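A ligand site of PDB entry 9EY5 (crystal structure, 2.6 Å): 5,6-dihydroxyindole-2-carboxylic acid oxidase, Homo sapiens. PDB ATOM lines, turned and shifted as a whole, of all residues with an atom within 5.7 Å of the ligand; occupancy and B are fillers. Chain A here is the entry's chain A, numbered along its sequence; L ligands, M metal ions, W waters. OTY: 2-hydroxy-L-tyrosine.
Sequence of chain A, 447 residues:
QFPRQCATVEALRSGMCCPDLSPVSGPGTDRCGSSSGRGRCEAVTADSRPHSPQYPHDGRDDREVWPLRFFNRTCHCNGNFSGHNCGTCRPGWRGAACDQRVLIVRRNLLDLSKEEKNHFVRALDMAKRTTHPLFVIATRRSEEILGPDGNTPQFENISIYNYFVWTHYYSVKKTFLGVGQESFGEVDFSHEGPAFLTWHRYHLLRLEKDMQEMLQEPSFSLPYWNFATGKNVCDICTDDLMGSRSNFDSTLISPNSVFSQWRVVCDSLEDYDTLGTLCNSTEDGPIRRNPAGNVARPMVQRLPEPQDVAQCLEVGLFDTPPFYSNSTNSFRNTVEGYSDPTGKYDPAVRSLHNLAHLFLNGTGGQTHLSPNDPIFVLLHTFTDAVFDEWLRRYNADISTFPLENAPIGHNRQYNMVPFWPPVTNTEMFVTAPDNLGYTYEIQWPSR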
ATOM      1  N   HIS A 168      22.712   5.435  24.283  1.00  0.00           N
ATOM      2  CA  HIS A 168      23.231   6.775  24.569  1.00  0.00           C
ATOM      3  C   HIS A 168      23.014   7.153  26.030  1.00  0.00           C
ATOM      4  O   HIS A 168      23.903   7.740  26.670  1.00  0.00           O
ATOM      5  CB  HIS A 168      22.571   7.761  23.622  1.00  0.00           C
ATOM      6  CG  HIS A 168      23.169   9.125  23.637  1.00  0.00           C
ATOM      7  ND1 HIS A 168      22.856  10.071  24.594  1.00  0.00           N
ATOM      8  CD2 HIS A 168      24.003   9.743  22.757  1.00  0.00           C
ATOM      9  CE1 HIS A 168      23.491  11.200  24.320  1.00  0.00           C
ATOM     10  NE2 HIS A 168      24.194  11.021  23.217  1.00  0.00           N
ATOM     11  N   HIS A 191      31.125  11.559  25.672  1.00  0.00           N
ATOM     12  CA  HIS A 191      31.360  12.974  25.439  1.00  0.00           C
ATOM     13  C   HIS A 191      32.504  13.428  26.311  1.00  0.00           C
ATOM     14  O   HIS A 191      32.924  12.723  27.238  1.00  0.00           O
ATOM     15  CB  HIS A 191      30.132  13.821  25.745  1.00  0.00           C
ATOM     16  CG  HIS A 191      28.858  13.185  25.289  1.00  0.00           C
ATOM     17  ND1 HIS A 191      28.261  12.149  25.964  1.00  0.00           N
ATOM     18  CD2 HIS A 191      28.112  13.402  24.182  1.00  0.00           C
ATOM     19  CE1 HIS A 191      27.180  11.771  25.313  1.00  0.00           C
ATOM     20  NE2 HIS A 191      27.057  12.523  24.235  1.00  0.00           N
ATOM     21  N   GLU A 192      33.011  14.627  26.008  1.00  0.00           N
ATOM     22  CA  GLU A 192      34.037  15.307  26.806  1.00  0.00           C
ATOM     23  C   GLU A 192      35.296  14.438  26.905  1.00  0.00           C
ATOM     24  O   GLU A 192      35.725  14.007  27.992  1.00  0.00           O
ATOM     25  CB  GLU A 192      33.471  15.674  28.176  1.00  0.00           C
ATOM     26  CG  GLU A 192      32.275  16.592  28.046  1.00  0.00           C
ATOM     27  CD  GLU A 192      31.512  16.767  29.327  1.00  0.00           C
ATOM     28  OE1 GLU A 192      32.092  17.289  30.309  1.00  0.00           O
ATOM     29  OE2 GLU A 192      30.315  16.365  29.346  1.00  0.00           O
ATOM     30  N   TYR A 338      33.220  22.548  22.763  1.00  0.00           N
ATOM     31  CA  TYR A 338      33.621  23.240  23.989  1.00  0.00           C
ATOM     32  C   TYR A 338      34.780  24.219  23.766  1.00  0.00           C
ATOM     33  O   TYR A 338      35.020  25.059  24.633  1.00  0.00           O
ATOM     34  CB  TYR A 338      34.015  22.255  25.075  1.00  0.00           C
ATOM     35  CG  TYR A 338      32.897  21.400  25.589  1.00  0.00           C
ATOM     36  CD1 TYR A 338      31.991  21.891  26.514  1.00  0.00           C
ATOM     37  CD2 TYR A 338      32.772  20.062  25.163  1.00  0.00           C
ATOM     38  CE1 TYR A 338      30.967  21.086  27.008  1.00  0.00           C
ATOM     39  CE2 TYR A 338      31.741  19.256  25.650  1.00  0.00           C
ATOM     40  CZ  TYR A 338      30.837  19.784  26.578  1.00  0.00           C
ATOM     41  OH  TYR A 338      29.819  19.026  27.085  1.00  0.00           O
ATOM     42  N   ARG A 350      30.233  28.030  23.306  1.00  0.00           N
ATOM     43  CA  ARG A 350      29.480  26.851  22.875  1.00  0.00           C
ATOM     44  C   ARG A 350      29.393  26.908  21.366  1.00  0.00           C
ATOM     45  O   ARG A 350      28.795  27.832  20.817  1.00  0.00           O
ATOM     46  CB  ARG A 350      28.079  26.812  23.495  1.00  0.00           C
ATOM     47  CG  ARG A 350      28.061  26.666  25.014  1.00  0.00           C
ATOM     48  CD  ARG A 350      29.164  25.708  25.434  1.00  0.00           C
ATOM     49  NE  ARG A 350      28.995  25.195  26.785  1.00  0.00           N
ATOM     50  CZ  ARG A 350      29.971  25.143  27.680  1.00  0.00           C
ATOM     51  NH1 ARG A 350      31.185  25.602  27.401  1.00  0.00           N
ATOM     52  NH2 ARG A 350      29.718  24.615  28.873  1.00  0.00           N
ATOM     53  N   HIS A 353      28.835  21.274  17.246  1.00  0.00           N
ATOM     54  CA  HIS A 353      27.927  20.199  17.668  1.00  0.00           C
ATOM     55  C   HIS A 353      27.183  20.569  18.944  1.00  0.00           C
ATOM     56  O   HIS A 353      25.969  20.320  19.047  1.00  0.00           O
ATOM     57  CB  HIS A 353      28.696  18.883  17.872  1.00  0.00           C
ATOM     58  CG  HIS A 353      28.122  17.983  18.940  1.00  0.00           C
ATOM     59  ND1 HIS A 353      28.371  18.178  20.286  1.00  0.00           N
ATOM     60  CD2 HIS A 353      27.319  16.896  18.869  1.00  0.00           C
ATOM     61  CE1 HIS A 353      27.751  17.252  20.988  1.00  0.00           C
ATOM     62  NE2 HIS A 353      27.123  16.463  20.158  1.00  0.00           N
ATOM     63  N   ASN A 354      27.873  21.141  19.933  1.00  0.00           N
ATOM     64  CA  ASN A 354      27.189  21.536  21.171  1.00  0.00           C
ATOM     65  C   ASN A 354      26.224  22.671  20.918  1.00  0.00           C
ATOM     66  O   ASN A 354      25.104  22.673  21.446  1.00  0.00           O
ATOM     67  CB  ASN A 354      28.192  21.953  22.252  1.00  0.00           C
ATOM     68  CG  ASN A 354      28.844  20.769  22.934  1.00  0.00           C
ATOM     69  OD1 ASN A 354      28.298  19.657  22.941  1.00  0.00           O
ATOM     70  ND2 ASN A 354      30.020  21.001  23.507  1.00  0.00           N
ATOM     71  N   HIS A 357      22.917  21.366  19.355  1.00  0.00           N
ATOM     72  CA  HIS A 357      22.009  20.800  20.342  1.00  0.00           C
ATOM     73  C   HIS A 357      21.243  21.880  21.109  1.00  0.00           C
ATOM     74  O   HIS A 357      20.023  21.827  21.232  1.00  0.00           O
ATOM     75  CB  HIS A 357      22.789  19.944  21.325  1.00  0.00           C
ATOM     76  CG  HIS A 357      23.008  18.546  20.881  1.00  0.00           C
ATOM     77  ND1 HIS A 357      22.126  17.520  21.180  1.00  0.00           N
ATOM     78  CD2 HIS A 357      24.024  17.978  20.209  1.00  0.00           C
ATOM     79  CE1 HIS A 357      22.590  16.393  20.685  1.00  0.00           C
ATOM     80  NE2 HIS A 357      23.733  16.640  20.079  1.00  0.00           N
ATOM     81  N   LEU A 358      21.962  22.869  21.674  1.00  0.00           N
ATOM     82  CA  LEU A 358      21.327  23.873  22.527  1.00  0.00           C
ATOM     83  C   LEU A 358      20.312  24.713  21.741  1.00  0.00           C
ATOM     84  O   LEU A 358      19.225  25.032  22.253  1.00  0.00           O
ATOM     85  CB  LEU A 358      22.394  24.763  23.151  1.00  0.00           C
ATOM     86  CG  LEU A 358      23.332  24.016  24.122  1.00  0.00           C
ATOM     87  CD1 LEU A 358      24.690  24.695  24.297  1.00  0.00           C
ATOM     88  CD2 LEU A 358      22.675  23.730  25.470  1.00  0.00           C
ATOM     89  N   GLY A 364      15.992  17.747  22.585  1.00  0.00           N
ATOM     90  CA  GLY A 364      17.222  17.565  21.827  1.00  0.00           C
ATOM     91  C   GLY A 364      18.474  18.115  22.483  1.00  0.00           C
ATOM     92  O   GLY A 364      19.555  18.012  21.902  1.00  0.00           O
ATOM     93  N   GLY A 365      18.364  18.678  23.680  1.00  0.00           N
ATOM     94  CA  GLY A 365      19.489  19.338  24.296  1.00  0.00           C
ATOM     95  C   GLY A 365      19.896  18.702  25.608  1.00  0.00           C
ATOM     96  O   GLY A 365      21.024  18.853  26.060  1.00  0.00           O
ATOM     97  N   GLN A 366      18.988  17.959  26.216  1.00  0.00           N
ATOM     98  CA  GLN A 366      19.300  17.280  27.462  1.00  0.00           C
ATOM     99  C   GLN A 366      20.159  16.036  27.185  1.00  0.00           C
ATOM    100  O   GLN A 366      19.761  15.152  26.415  1.00  0.00           O
ATOM    101  CB  GLN A 366      17.994  16.929  28.156  1.00  0.00           C
ATOM    102  CG  GLN A 366      16.939  18.009  27.876  1.00  0.00           C
ATOM    103  CD  GLN A 366      15.692  17.860  28.711  1.00  0.00           C
ATOM    104  OE1 GLN A 366      14.593  17.662  28.167  1.00  0.00           O
ATOM    105  NE2 GLN A 366      15.852  17.941  30.027  1.00  0.00           N
ATOM    106  N   THR A 367      21.340  15.955  27.822  1.00  0.00           N
ATOM    107  CA  THR A 367      22.321  14.960  27.394  1.00  0.00           C
ATOM    108  C   THR A 367      21.802  13.533  27.573  1.00  0.00           C
ATOM    109  O   THR A 367      22.123  12.664  26.749  1.00  0.00           O
ATOM    110  CB  THR A 367      23.649  15.143  28.140  1.00  0.00           C
ATOM    111  OG1 THR A 367      24.131  16.480  27.948  1.00  0.00           O
ATOM    112  CG2 THR A 367      24.719  14.101  27.620  1.00  0.00           C
ATOM    113  N   HIS A 368      20.992  13.279  28.593  1.00  0.00           N
ATOM    114  CA  HIS A 368      20.473  11.924  28.741  1.00  0.00           C
ATOM    115  C   HIS A 368      19.266  11.639  27.837  1.00  0.00           C
ATOM    116  O   HIS A 368      18.905  10.469  27.669  1.00  0.00           O
ATOM    117  CB  HIS A 368      20.081  11.652  30.206  1.00  0.00           C
ATOM    118  CG  HIS A 368      18.923  12.467  30.679  1.00  0.00           C
ATOM    119  ND1 HIS A 368      18.958  13.843  30.728  1.00  0.00           N
ATOM    120  CD2 HIS A 368      17.684  12.101  31.093  1.00  0.00           C
ATOM    121  CE1 HIS A 368      17.794  14.286  31.175  1.00  0.00           C
ATOM    122  NE2 HIS A 368      17.006  13.254  31.408  1.00  0.00           N
ATOM    123  N   SER A 370      18.682  13.373  24.560  1.00  0.00           N
ATOM    124  CA  SER A 370      18.698  14.025  23.248  1.00  0.00           C
ATOM    125  C   SER A 370      18.364  13.127  22.057  1.00  0.00           C
ATOM    126  O   SER A 370      17.651  13.601  21.161  1.00  0.00           O
ATOM    127  CB  SER A 370      20.055  14.714  23.032  1.00  0.00           C
ATOM    128  OG  SER A 370      21.101  13.882  23.483  1.00  0.00           O
ATOM    129  N   PRO A 371      18.811  11.864  21.970  1.00  0.00           N
ATOM    130  CA  PRO A 371      18.437  11.050  20.787  1.00  0.00           C
ATOM    131  C   PRO A 371      16.931  10.843  20.614  1.00  0.00           C
ATOM    132  O   PRO A 371      16.528  10.345  19.549  1.00  0.00           O
ATOM    133  CB  PRO A 371      19.157   9.716  21.029  1.00  0.00           C
ATOM    134  CG  PRO A 371      20.192   9.997  22.036  1.00  0.00           C
ATOM    135  CD  PRO A 371      19.686  11.103  22.880  1.00  0.00           C
ATOM    136  N   PHE A 376      18.484  14.398  16.212  1.00  0.00           N
ATOM    137  CA  PHE A 376      19.742  13.860  16.727  1.00  0.00           C
ATOM    138  C   PHE A 376      20.487  13.106  15.636  1.00  0.00           C
ATOM    139  O   PHE A 376      21.680  13.329  15.402  1.00  0.00           O
ATOM    140  CB  PHE A 376      19.478  12.937  17.918  1.00  0.00           C
ATOM    141  CG  PHE A 376      20.731  12.415  18.580  1.00  0.00           C
ATOM    142  CD1 PHE A 376      21.489  11.410  17.993  1.00  0.00           C
ATOM    143  CD2 PHE A 376      21.166  12.950  19.793  1.00  0.00           C
ATOM    144  CE1 PHE A 376      22.665  10.939  18.591  1.00  0.00           C
ATOM    145  CE2 PHE A 376      22.339  12.484  20.407  1.00  0.00           C
ATOM    146  CZ  PHE A 376      23.083  11.475  19.806  1.00  0.00           C
HETATM  147  OD1 OTY L   1      23.011  19.785  25.067  1.00  0.00           O
HETATM  148  N   OTY L   1      26.929  21.796  26.503  1.00  0.00           N
HETATM  149  CA  OTY L   1      25.835  20.848  26.222  1.00  0.00           C
HETATM  150  C   OTY L   1      25.865  19.679  27.228  1.00  0.00           C
HETATM  151  O   OTY L   1      24.787  19.279  27.758  1.00  0.00           O
HETATM  152  CB  OTY L   1      25.914  20.314  24.733  1.00  0.00           C
HETATM  153  CG  OTY L   1      25.266  18.908  24.519  1.00  0.00           C
HETATM  154  CD1 OTY L   1      23.895  18.703  24.685  1.00  0.00           C
HETATM  155  CD2 OTY L   1      26.062  17.782  24.122  1.00  0.00           C
HETATM  156  CE1 OTY L   1      23.297  17.408  24.483  1.00  0.00           C
HETATM  157  CE2 OTY L   1      25.507  16.482  23.934  1.00  0.00           C
HETATM  158  CZ  OTY L   1      24.112  16.318  24.115  1.00  0.00           C
HETATM  159  OH  OTY L   1      23.475  15.020  23.924  1.00  0.00           O
HETATM  160  OXT OTY L   1      26.966  19.102  27.537  1.00  0.00           O
HETATM  161 ZN    ZN M   1      25.796  12.331  22.400  1.00  0.00          ZN
HETATM  162 ZN    ZN M   2      25.379  15.129  20.288  1.00  0.00          ZN
HETATM  163  O   HOH W   1      29.127  16.919  24.162  1.00  0.00           O
HETATM  164  O   HOH W   2      27.759  16.544  26.565  1.00  0.00           O
HETATM  165  O   HOH W   3      25.003  14.100  21.789  1.00  0.00           O
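An oxygen (OD1) of the ligand sits at hydrogen-bond distance from the backbone carbonyl oxygen (O) of Gly 365, at 2.4 Å. An oxygen (OH) of the ligand sits at hydrogen-bond distance from the side-chain hydroxyl (OG) of Ser 370 (2.7 Å). An oxygen (O) of the ligand is in hydrogen-bond range of the side-chain hydroxyl (OG1) of Thr 367, 2.9 Å away. OH of Tyr 338 is in hydrogen-bond range of OXT of the ligand, at 2.9 Å.
OG of Ser 370 sits close to O of Gln 366 (3.5 Å). The backbone carbonyl oxygen (O) of Thr 367 lies close to a ring nitrogen (ND1) of His 168. The side-chain amide oxygen (OD1) of Asn 354 sits at hydrogen-bond distance from a ring nitrogen (ND1) of His 353 (3.0 Å). O of Gly 364 is in hydrogen-bond range of ND1 of His 357, 2.7 Å away.
Residues that only touch the ligand: His 168 (3.8 Å), Arg 350 (3.99 Å), His 353 (3.6 Å), Asn 354 (3.1 Å), His 357 (3.5 Å) and Leu 358 (3.98 Å). Hydrophobic or aromatic side chains within 4 Å of the ligand: His 168, His 353, His 357 and Leu 358. Ten residues have an atom within 4 Å of the ligand: His 168, Tyr 338, Arg 350, His 353, Asn 354, His 357, Leu 358, Gly 365, Thr 367 and Ser 370.
Water W2 lies within hydrogen-bond range of an oxygen (OXT) of the ligand (2.8 Å) and the side-chain hydroxyl of Tyr 338 (3.3 Å).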
